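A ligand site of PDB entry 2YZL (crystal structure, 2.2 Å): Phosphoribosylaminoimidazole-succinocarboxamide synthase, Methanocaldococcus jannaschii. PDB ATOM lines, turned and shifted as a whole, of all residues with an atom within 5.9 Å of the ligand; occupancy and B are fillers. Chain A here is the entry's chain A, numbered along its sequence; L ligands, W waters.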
ATOM      1  N   TYR A  15     -22.943   0.706  29.230  1.00  0.00           N
ATOM      2  CA  TYR A  15     -23.047   1.997  29.898  1.00  0.00           C
ATOM      3  C   TYR A  15     -23.788   2.987  29.020  1.00  0.00           C
ATOM      4  O   TYR A  15     -23.626   3.008  27.807  1.00  0.00           O
ATOM      5  CB  TYR A  15     -21.664   2.558  30.206  1.00  0.00           C
ATOM      6  CG  TYR A  15     -21.746   3.932  30.833  1.00  0.00           C
ATOM      7  CD1 TYR A  15     -22.198   4.092  32.143  1.00  0.00           C
ATOM      8  CD2 TYR A  15     -21.432   5.074  30.094  1.00  0.00           C
ATOM      9  CE1 TYR A  15     -22.338   5.353  32.705  1.00  0.00           C
ATOM     10  CE2 TYR A  15     -21.581   6.337  30.646  1.00  0.00           C
ATOM     11  CZ  TYR A  15     -22.029   6.472  31.946  1.00  0.00           C
ATOM     12  OH  TYR A  15     -22.189   7.726  32.496  1.00  0.00           O
ATOM     13  N   SER A  16     -24.616   3.814  29.651  1.00  0.00           N
ATOM     14  CA  SER A  16     -25.378   4.837  28.946  1.00  0.00           C
ATOM     15  C   SER A  16     -25.145   6.168  29.632  1.00  0.00           C
ATOM     16  O   SER A  16     -25.332   6.283  30.845  1.00  0.00           O
ATOM     17  CB  SER A  16     -26.873   4.517  28.971  1.00  0.00           C
ATOM     18  OG  SER A  16     -27.163   3.335  28.240  1.00  0.00           O
ATOM     19  N   GLY A  17     -24.712   7.175  28.870  1.00  0.00           N
ATOM     20  CA  GLY A  17     -24.470   8.475  29.467  1.00  0.00           C
ATOM     21  C   GLY A  17     -25.437   9.531  28.968  1.00  0.00           C
ATOM     22  O   GLY A  17     -26.487   9.204  28.428  1.00  0.00           O
ATOM     23  N   LYS A  18     -25.077  10.795  29.129  1.00  0.00           N
ATOM     24  CA  LYS A  18     -25.931  11.892  28.701  1.00  0.00           C
ATOM     25  C   LYS A  18     -25.948  12.117  27.191  1.00  0.00           C
ATOM     26  O   LYS A  18     -26.823  12.828  26.681  1.00  0.00           O
ATOM     27  CB  LYS A  18     -25.500  13.202  29.374  1.00  0.00           C
ATOM     28  CG  LYS A  18     -25.461  13.145  30.876  1.00  0.00           C
ATOM     29  CD  LYS A  18     -25.128  14.512  31.470  1.00  0.00           C
ATOM     30  CE  LYS A  18     -23.748  14.988  31.030  1.00  0.00           C
ATOM     31  NZ  LYS A  18     -22.666  14.115  31.554  1.00  0.00           N
ATOM     32  N   ALA A  19     -24.996  11.537  26.470  1.00  0.00           N
ATOM     33  CA  ALA A  19     -24.953  11.747  25.019  1.00  0.00           C
ATOM     34  C   ALA A  19     -24.735  10.502  24.166  1.00  0.00           C
ATOM     35  O   ALA A  19     -25.081  10.484  22.985  1.00  0.00           O
ATOM     36  CB  ALA A  19     -23.868  12.776  24.688  1.00  0.00           C
ATOM     37  N   LYS A  20     -24.162   9.459  24.759  1.00  0.00           N
ATOM     38  CA  LYS A  20     -23.896   8.240  24.009  1.00  0.00           C
ATOM     39  C   LYS A  20     -24.146   6.952  24.786  1.00  0.00           C
ATOM     40  O   LYS A  20     -24.294   6.970  26.005  1.00  0.00           O
ATOM     41  CB  LYS A  20     -22.443   8.241  23.510  1.00  0.00           C
ATOM     42  CG  LYS A  20     -22.048   9.476  22.705  1.00  0.00           C
ATOM     43  CD  LYS A  20     -20.675   9.313  22.070  1.00  0.00           C
ATOM     44  CE  LYS A  20     -19.556   9.187  23.095  1.00  0.00           C
ATOM     45  NZ  LYS A  20     -19.319  10.426  23.895  1.00  0.00           N
ATOM     46  N   SER A  21     -24.194   5.840  24.064  1.00  0.00           N
ATOM     47  CA  SER A  21     -24.395   4.528  24.673  1.00  0.00           C
ATOM     48  C   SER A  21     -23.291   3.598  24.216  1.00  0.00           C
ATOM     49  O   SER A  21     -22.956   3.542  23.043  1.00  0.00           O
ATOM     50  CB  SER A  21     -25.744   3.920  24.247  1.00  0.00           C
ATOM     51  OG  SER A  21     -26.847   4.641  24.779  1.00  0.00           O
ATOM     52  N   ILE A  22     -22.724   2.874  25.178  1.00  0.00           N
ATOM     53  CA  ILE A  22     -21.658   1.922  24.876  1.00  0.00           C
ATOM     54  C   ILE A  22     -22.247   0.508  24.888  1.00  0.00           C
ATOM     55  O   ILE A  22     -22.726   0.045  25.925  1.00  0.00           O
ATOM     56  CB  ILE A  22     -20.516   1.996  25.912  1.00  0.00           C
ATOM     57  CG1 ILE A  22     -19.806   3.356  25.845  1.00  0.00           C
ATOM     58  CG2 ILE A  22     -19.481   0.920  25.618  1.00  0.00           C
ATOM     59  CD1 ILE A  22     -20.647   4.527  26.367  1.00  0.00           C
ATOM     60  N   VAL A  30     -16.017  -2.291  21.411  1.00  0.00           N
ATOM     61  CA  VAL A  30     -17.352  -1.816  21.733  1.00  0.00           C
ATOM     62  C   VAL A  30     -17.966  -1.038  20.587  1.00  0.00           C
ATOM     63  O   VAL A  30     -17.278  -0.606  19.658  1.00  0.00           O
ATOM     64  CB  VAL A  30     -17.338  -0.879  22.965  1.00  0.00           C
ATOM     65  CG1 VAL A  30     -17.032  -1.663  24.226  1.00  0.00           C
ATOM     66  CG2 VAL A  30     -16.325   0.245  22.753  1.00  0.00           C
ATOM     67  N   ILE A  32     -20.109   2.302  19.908  1.00  0.00           N
ATOM     68  CA  ILE A  32     -20.508   3.545  20.554  1.00  0.00           C
ATOM     69  C   ILE A  32     -21.638   4.170  19.736  1.00  0.00           C
ATOM     70  O   ILE A  32     -21.503   4.363  18.525  1.00  0.00           O
ATOM     71  CB  ILE A  32     -19.344   4.570  20.634  1.00  0.00           C
ATOM     72  CG1 ILE A  32     -18.159   3.956  21.389  1.00  0.00           C
ATOM     73  CG2 ILE A  32     -19.828   5.820  21.348  1.00  0.00           C
ATOM     74  CD1 ILE A  32     -16.763   4.606  21.165  1.00  0.00           C
ATOM     75  N   ARG A  35     -26.091   9.398  20.388  1.00  0.00           N
ATOM     76  CA  ARG A  35     -27.511   9.744  20.393  1.00  0.00           C
ATOM     77  C   ARG A  35     -27.738  11.216  20.036  1.00  0.00           C
ATOM     78  O   ARG A  35     -26.789  11.995  19.909  1.00  0.00           O
ATOM     79  CB  ARG A  35     -28.133   9.434  21.759  1.00  0.00           C
ATOM     80  CG  ARG A  35     -27.941   7.997  22.243  1.00  0.00           C
ATOM     81  CD  ARG A  35     -28.935   7.628  23.345  1.00  0.00           C
ATOM     82  NE  ARG A  35     -28.913   8.598  24.443  1.00  0.00           N
ATOM     83  CZ  ARG A  35     -28.028   8.605  25.423  1.00  0.00           C
ATOM     84  NH1 ARG A  35     -27.070   7.687  25.487  1.00  0.00           N
ATOM     85  NH2 ARG A  35     -28.088   9.544  26.361  1.00  0.00           N
ATOM     86  N   HIS A  75      -8.822   4.992  20.129  1.00  0.00           N
ATOM     87  CA  HIS A  75      -9.640   3.791  20.276  1.00  0.00           C
ATOM     88  C   HIS A  75     -10.485   3.546  19.028  1.00  0.00           C
ATOM     89  O   HIS A  75     -11.214   2.566  18.950  1.00  0.00           O
ATOM     90  CB  HIS A  75     -10.548   3.934  21.511  1.00  0.00           C
ATOM     91  CG  HIS A  75     -11.713   4.869  21.334  1.00  0.00           C
ATOM     92  ND1 HIS A  75     -11.674   5.953  20.491  1.00  0.00           N
ATOM     93  CD2 HIS A  75     -12.923   4.900  21.933  1.00  0.00           C
ATOM     94  CE1 HIS A  75     -12.812   6.626  20.584  1.00  0.00           C
ATOM     95  NE2 HIS A  75     -13.583   5.999  21.453  1.00  0.00           N
ATOM     96  N   ALA A  87     -15.180   0.955  18.436  1.00  0.00           N
ATOM     97  CA  ALA A  87     -13.954   1.371  19.099  1.00  0.00           C
ATOM     98  C   ALA A  87     -13.323   0.275  19.936  1.00  0.00           C
ATOM     99  O   ALA A  87     -13.971  -0.715  20.285  1.00  0.00           O
ATOM    100  CB  ALA A  87     -14.241   2.598  19.975  1.00  0.00           C
ATOM    101  N   LYS A  88     -12.058   0.455  20.250  1.00  0.00           N
ATOM    102  CA  LYS A  88     -11.357  -0.500  21.086  1.00  0.00           C
ATOM    103  C   LYS A  88     -11.871  -0.217  22.492  1.00  0.00           C
ATOM    104  O   LYS A  88     -11.957   0.940  22.910  1.00  0.00           O
ATOM    105  CB  LYS A  88      -9.845  -0.265  21.031  1.00  0.00           C
ATOM    106  CG  LYS A  88      -9.209  -0.492  19.681  1.00  0.00           C
ATOM    107  CD  LYS A  88      -7.707  -0.241  19.754  1.00  0.00           C
ATOM    108  CE  LYS A  88      -7.034  -0.425  18.407  1.00  0.00           C
ATOM    109  NZ  LYS A  88      -5.543  -0.343  18.549  1.00  0.00           N
ATOM    110  N   LYS A  89     -12.233  -1.273  23.210  1.00  0.00           N
ATOM    111  CA  LYS A  89     -12.709  -1.114  24.573  1.00  0.00           C
ATOM    112  C   LYS A  89     -11.553  -0.729  25.494  1.00  0.00           C
ATOM    113  O   LYS A  89     -10.506  -1.374  25.509  1.00  0.00           O
ATOM    114  CB  LYS A  89     -13.352  -2.407  25.061  1.00  0.00           C
ATOM    115  CG  LYS A  89     -13.984  -2.302  26.426  1.00  0.00           C
ATOM    116  CD  LYS A  89     -14.663  -3.602  26.805  1.00  0.00           C
ATOM    117  CE  LYS A  89     -15.362  -3.489  28.148  1.00  0.00           C
ATOM    118  NZ  LYS A  89     -16.083  -4.741  28.490  1.00  0.00           N
ATOM    119  N   VAL A  90     -11.748   0.341  26.256  1.00  0.00           N
ATOM    120  CA  VAL A  90     -10.712   0.800  27.163  1.00  0.00           C
ATOM    121  C   VAL A  90     -11.324   1.086  28.526  1.00  0.00           C
ATOM    122  O   VAL A  90     -12.536   1.215  28.661  1.00  0.00           O
ATOM    123  CB  VAL A  90     -10.034   2.106  26.674  1.00  0.00           C
ATOM    124  CG1 VAL A  90      -9.523   1.945  25.253  1.00  0.00           C
ATOM    125  CG2 VAL A  90     -11.019   3.265  26.764  1.00  0.00           C
ATOM    126  N   GLU A  91     -10.473   1.178  29.532  1.00  0.00           N
ATOM    127  CA  GLU A  91     -10.899   1.508  30.871  1.00  0.00           C
ATOM    128  C   GLU A  91     -10.552   2.992  30.980  1.00  0.00           C
ATOM    129  O   GLU A  91      -9.373   3.356  31.041  1.00  0.00           O
ATOM    130  CB  GLU A  91     -10.123   0.660  31.886  1.00  0.00           C
ATOM    131  CG  GLU A  91     -10.642   0.750  33.306  1.00  0.00           C
ATOM    132  CD  GLU A  91     -10.138  -0.376  34.193  1.00  0.00           C
ATOM    133  OE1 GLU A  91     -10.380  -1.554  33.844  1.00  0.00           O
ATOM    134  OE2 GLU A  91      -9.506  -0.092  35.237  1.00  0.00           O
ATOM    135  N   ILE A  92     -11.574   3.835  30.962  1.00  0.00           N
ATOM    136  CA  ILE A  92     -11.362   5.281  31.024  1.00  0.00           C
ATOM    137  C   ILE A  92     -10.750   5.778  32.330  1.00  0.00           C
ATOM    138  O   ILE A  92     -11.149   5.365  33.422  1.00  0.00           O
ATOM    139  CB  ILE A  92     -12.689   6.064  30.786  1.00  0.00           C
ATOM    140  CG1 ILE A  92     -13.087   5.999  29.308  1.00  0.00           C
ATOM    141  CG2 ILE A  92     -12.526   7.522  31.157  1.00  0.00           C
ATOM    142  CD1 ILE A  92     -12.198   6.810  28.370  1.00  0.00           C
ATOM    143  N   LYS A 129     -13.061  13.868  36.765  1.00  0.00           N
ATOM    144  CA  LYS A 129     -14.402  13.521  36.288  1.00  0.00           C
ATOM    145  C   LYS A 129     -15.123  12.832  37.437  1.00  0.00           C
ATOM    146  O   LYS A 129     -14.995  11.626  37.639  1.00  0.00           O
ATOM    147  CB  LYS A 129     -14.337  12.597  35.072  1.00  0.00           C
ATOM    148  CG  LYS A 129     -15.643  12.521  34.286  1.00  0.00           C
ATOM    149  CD  LYS A 129     -15.546  11.586  33.085  1.00  0.00           C
ATOM    150  CE  LYS A 129     -16.849  11.564  32.300  1.00  0.00           C
ATOM    151  NZ  LYS A 129     -16.876  10.524  31.238  1.00  0.00           N
ATOM    152  N   GLU A 185     -10.699  12.442  26.492  1.00  0.00           N
ATOM    153  CA  GLU A 185     -10.647  11.481  27.574  1.00  0.00           C
ATOM    154  C   GLU A 185      -9.692  10.393  27.133  1.00  0.00           C
ATOM    155  O   GLU A 185      -9.611  10.052  25.946  1.00  0.00           O
ATOM    156  CB  GLU A 185     -12.032  10.889  27.845  1.00  0.00           C
ATOM    157  CG  GLU A 185     -12.873  11.742  28.783  1.00  0.00           C
ATOM    158  CD  GLU A 185     -14.273  11.182  28.974  1.00  0.00           C
ATOM    159  OE1 GLU A 185     -14.434   9.947  28.846  1.00  0.00           O
ATOM    160  OE2 GLU A 185     -15.193  11.972  29.268  1.00  0.00           O
ATOM    161  N   ALA A 197      -9.721   8.264  23.825  1.00  0.00           N
ATOM    162  CA  ALA A 197     -11.007   7.594  23.647  1.00  0.00           C
ATOM    163  C   ALA A 197     -12.139   8.584  23.441  1.00  0.00           C
ATOM    164  O   ALA A 197     -11.957   9.661  22.870  1.00  0.00           O
ATOM    165  CB  ALA A 197     -11.281   6.705  24.852  1.00  0.00           C
ATOM    166  N   ASP A 198     -13.318   8.192  23.915  1.00  0.00           N
ATOM    167  CA  ASP A 198     -14.528   9.012  23.814  1.00  0.00           C
ATOM    168  C   ASP A 198     -14.744   9.598  22.429  1.00  0.00           C
ATOM    169  O   ASP A 198     -14.769   8.864  21.448  1.00  0.00           O
ATOM    170  CB  ASP A 198     -14.484  10.124  24.857  1.00  0.00           C
ATOM    171  CG  ASP A 198     -15.867  10.644  25.199  1.00  0.00           C
ATOM    172  OD1 ASP A 198     -16.098  11.876  25.088  1.00  0.00           O
ATOM    173  OD2 ASP A 198     -16.726   9.826  25.583  1.00  0.00           O
ATOM    174  N   GLU A 199     -14.902  10.916  22.339  1.00  0.00           N
ATOM    175  CA  GLU A 199     -15.136  11.567  21.051  1.00  0.00           C
ATOM    176  C   GLU A 199     -14.441  12.918  20.946  1.00  0.00           C
ATOM    177  O   GLU A 199     -14.021  13.491  21.946  1.00  0.00           O
ATOM    178  CB  GLU A 199     -16.636  11.818  20.846  1.00  0.00           C
ATOM    179  CG  GLU A 199     -17.215  12.821  21.845  1.00  0.00           C
ATOM    180  CD  GLU A 199     -18.696  13.096  21.627  1.00  0.00           C
ATOM    181  OE1 GLU A 199     -19.033  13.783  20.647  1.00  0.00           O
ATOM    182  OE2 GLU A 199     -19.512  12.614  22.446  1.00  0.00           O
HETATM  183  P1  LIG L   1     -21.216  10.885  30.210  1.00  0.00           P
HETATM  184  O1  LIG L   1     -21.201   9.419  30.199  1.00  0.00           O
HETATM  185  O2  LIG L   1     -22.274  11.792  29.425  1.00  0.00           O
HETATM  186  O3  LIG L   1     -19.856  11.653  30.626  1.00  0.00           O
HETATM  187  P2  LIG L   1     -21.403  10.482  27.433  1.00  0.00           P
HETATM  188  O4  LIG L   1     -20.719  10.533  26.119  1.00  0.00           O
HETATM  189  O5  LIG L   1     -22.871   9.882  27.622  1.00  0.00           O
HETATM  190  O6  LIG L   1     -20.429  10.642  28.764  1.00  0.00           O
HETATM  191  O7  LIG L   1     -21.054   8.875  27.447  1.00  0.00           O
HETATM  192  C1  LIG L   1     -19.656   8.597  27.196  1.00  0.00           C
HETATM  193  C2  LIG L   1     -19.211   7.479  28.134  1.00  0.00           C
HETATM  194  O8  LIG L   1     -18.612   6.391  27.368  1.00  0.00           O
HETATM  195  C3  LIG L   1     -18.159   7.985  29.120  1.00  0.00           C
HETATM  196  O9  LIG L   1     -18.496   7.559  30.452  1.00  0.00           O
HETATM  197  C4  LIG L   1     -16.851   7.382  28.596  1.00  0.00           C
HETATM  198  O10 LIG L   1     -15.919   7.202  29.652  1.00  0.00           O
HETATM  199  C5  LIG L   1     -17.323   6.073  27.943  1.00  0.00           C
HETATM  200  N1  LIG L   1     -16.399   5.606  26.882  1.00  0.00           N
HETATM  201  C6  LIG L   1     -15.854   6.352  25.855  1.00  0.00           C
HETATM  202  N2  LIG L   1     -15.103   5.597  25.096  1.00  0.00           N
HETATM  203  C7  LIG L   1     -15.087   4.326  25.588  1.00  0.00           C
HETATM  204  C8  LIG L   1     -14.455   3.096  25.232  1.00  0.00           C
HETATM  205  N3  LIG L   1     -13.806   2.945  24.022  1.00  0.00           N
HETATM  206  N4  LIG L   1     -14.489   2.079  26.119  1.00  0.00           N
HETATM  207  C9  LIG L   1     -15.327   2.093  27.166  1.00  0.00           C
HETATM  208  N5  LIG L   1     -16.102   3.157  27.408  1.00  0.00           N
HETATM  209  C10 LIG L   1     -15.943   4.315  26.728  1.00  0.00           C
HETATM  210  O   HOH W   1     -23.300  10.679  32.286  1.00  0.00           O
HETATM  211  O   HOH W   2     -20.605  13.538  26.331  1.00  0.00           O
HETATM  212  O   HOH W   3     -17.628   2.359  29.670  1.00  0.00           O
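O5 of the ligand sits at hydrogen-bond distance from N of Lys 18. The backbone NH (N) of Asp 198 lies within hydrogen-bond range of a nitrogen (N2) of the ligand. The backbone carbonyl oxygen of Lys 88 lies within hydrogen-bond range of a nitrogen (N3) of the ligand, at 2.9 Å. An oxygen (O4) of the ligand is in salt-bridge range of the side-chain amino group (NZ) of Lys 20, at 2.6 Å. OE1 of Glu 185 is in hydrogen-bond range of O10 of the ligand, 3.2 Å away. N of Lys 20 is in hydrogen-bond range of O5 of the ligand. The backbone NH (N) of Val 90 is in hydrogen-bond range of a nitrogen (N4) of the ligand (3.2 Å). The backbone NH (N) of Ala 19 is in hydrogen-bond range of an oxygen (O5) of the ligand, at 2.9 Å. The side-chain amino group (NZ) of Lys 129 is in salt-bridge range of an oxygen (O3) of the ligand (3.2 Å). An oxygen (O2) of the ligand is in salt-bridge range of the side-chain amino group (NZ) of Lys 18. OH of Tyr 15 lies within hydrogen-bond range of O1 of the ligand, 3.0 Å away.
Water W1 lies within hydrogen-bond range of the side-chain hydroxyl of Tyr 15 (3.2 Å) and an oxygen (O1) of the ligand (3.2 Å).
The backbone carbonyl oxygen (O) of Gly 17 lies within hydrogen-bond range of the guanidinium group (NH2) of Arg 35, 2.6 Å away. The side-chain carboxylate of Glu 185 lies within salt-bridge range of the side-chain amino group of Lys 129. NZ of Lys 20 is in salt-bridge range of OE2 of Glu 199 (2.6 Å). The backbone carbonyl oxygen (O) of Glu 185 is in hydrogen-bond range of the backbone NH (N) of Ala 197 (2.8 Å). The backbone carbonyl oxygen (O) of Ala 87 is in hydrogen-bond range of the backbone NH (N) of Val 30 (2.8 Å). The backbone carbonyl oxygen of Asp 198 sits close to a ring nitrogen (NE2) of His 75. The backbone NH (N) of Arg 35 sits at hydrogen-bond distance from the backbone carbonyl oxygen (O) of Ala 19 (3.0 Å). The backbone carbonyl oxygen (O) of Lys 20 lies within hydrogen-bond range of the guanidinium group (NH1) of Arg 35, 2.9 Å away.
CA of Gly 17 touches O5 of the ligand, 2.8 Å away. Ile 22 touches the ligand. Val 30 touches the ligand (CG2 to N3, 3.9 Å). CD2 of His 75 touches N3 of the ligand, at 3.0 Å. CA of Lys 89 touches N4 of the ligand (3.97 Å). Ile 92 touches the ligand (CG1 to O10, 3.1 Å). CB of Ala 197 touches N2 of the ligand, at 3.99 Å. Hydrophobic or aromatic side chains within 4 Å of the ligand: Tyr 15, Ile 22, Val 30, His 75, Val 90, Ile 92 and Ala 197. 16 residues have an atom within 4 Å of the ligand: Tyr 15, Gly 17, Lys 18, Ala 19, Lys 20, Ile 22, Val 30, His 75, Lys 88, Lys 89, Val 90, Ile 92, Lys 129, Glu 185, Ala 197 and Asp 198.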
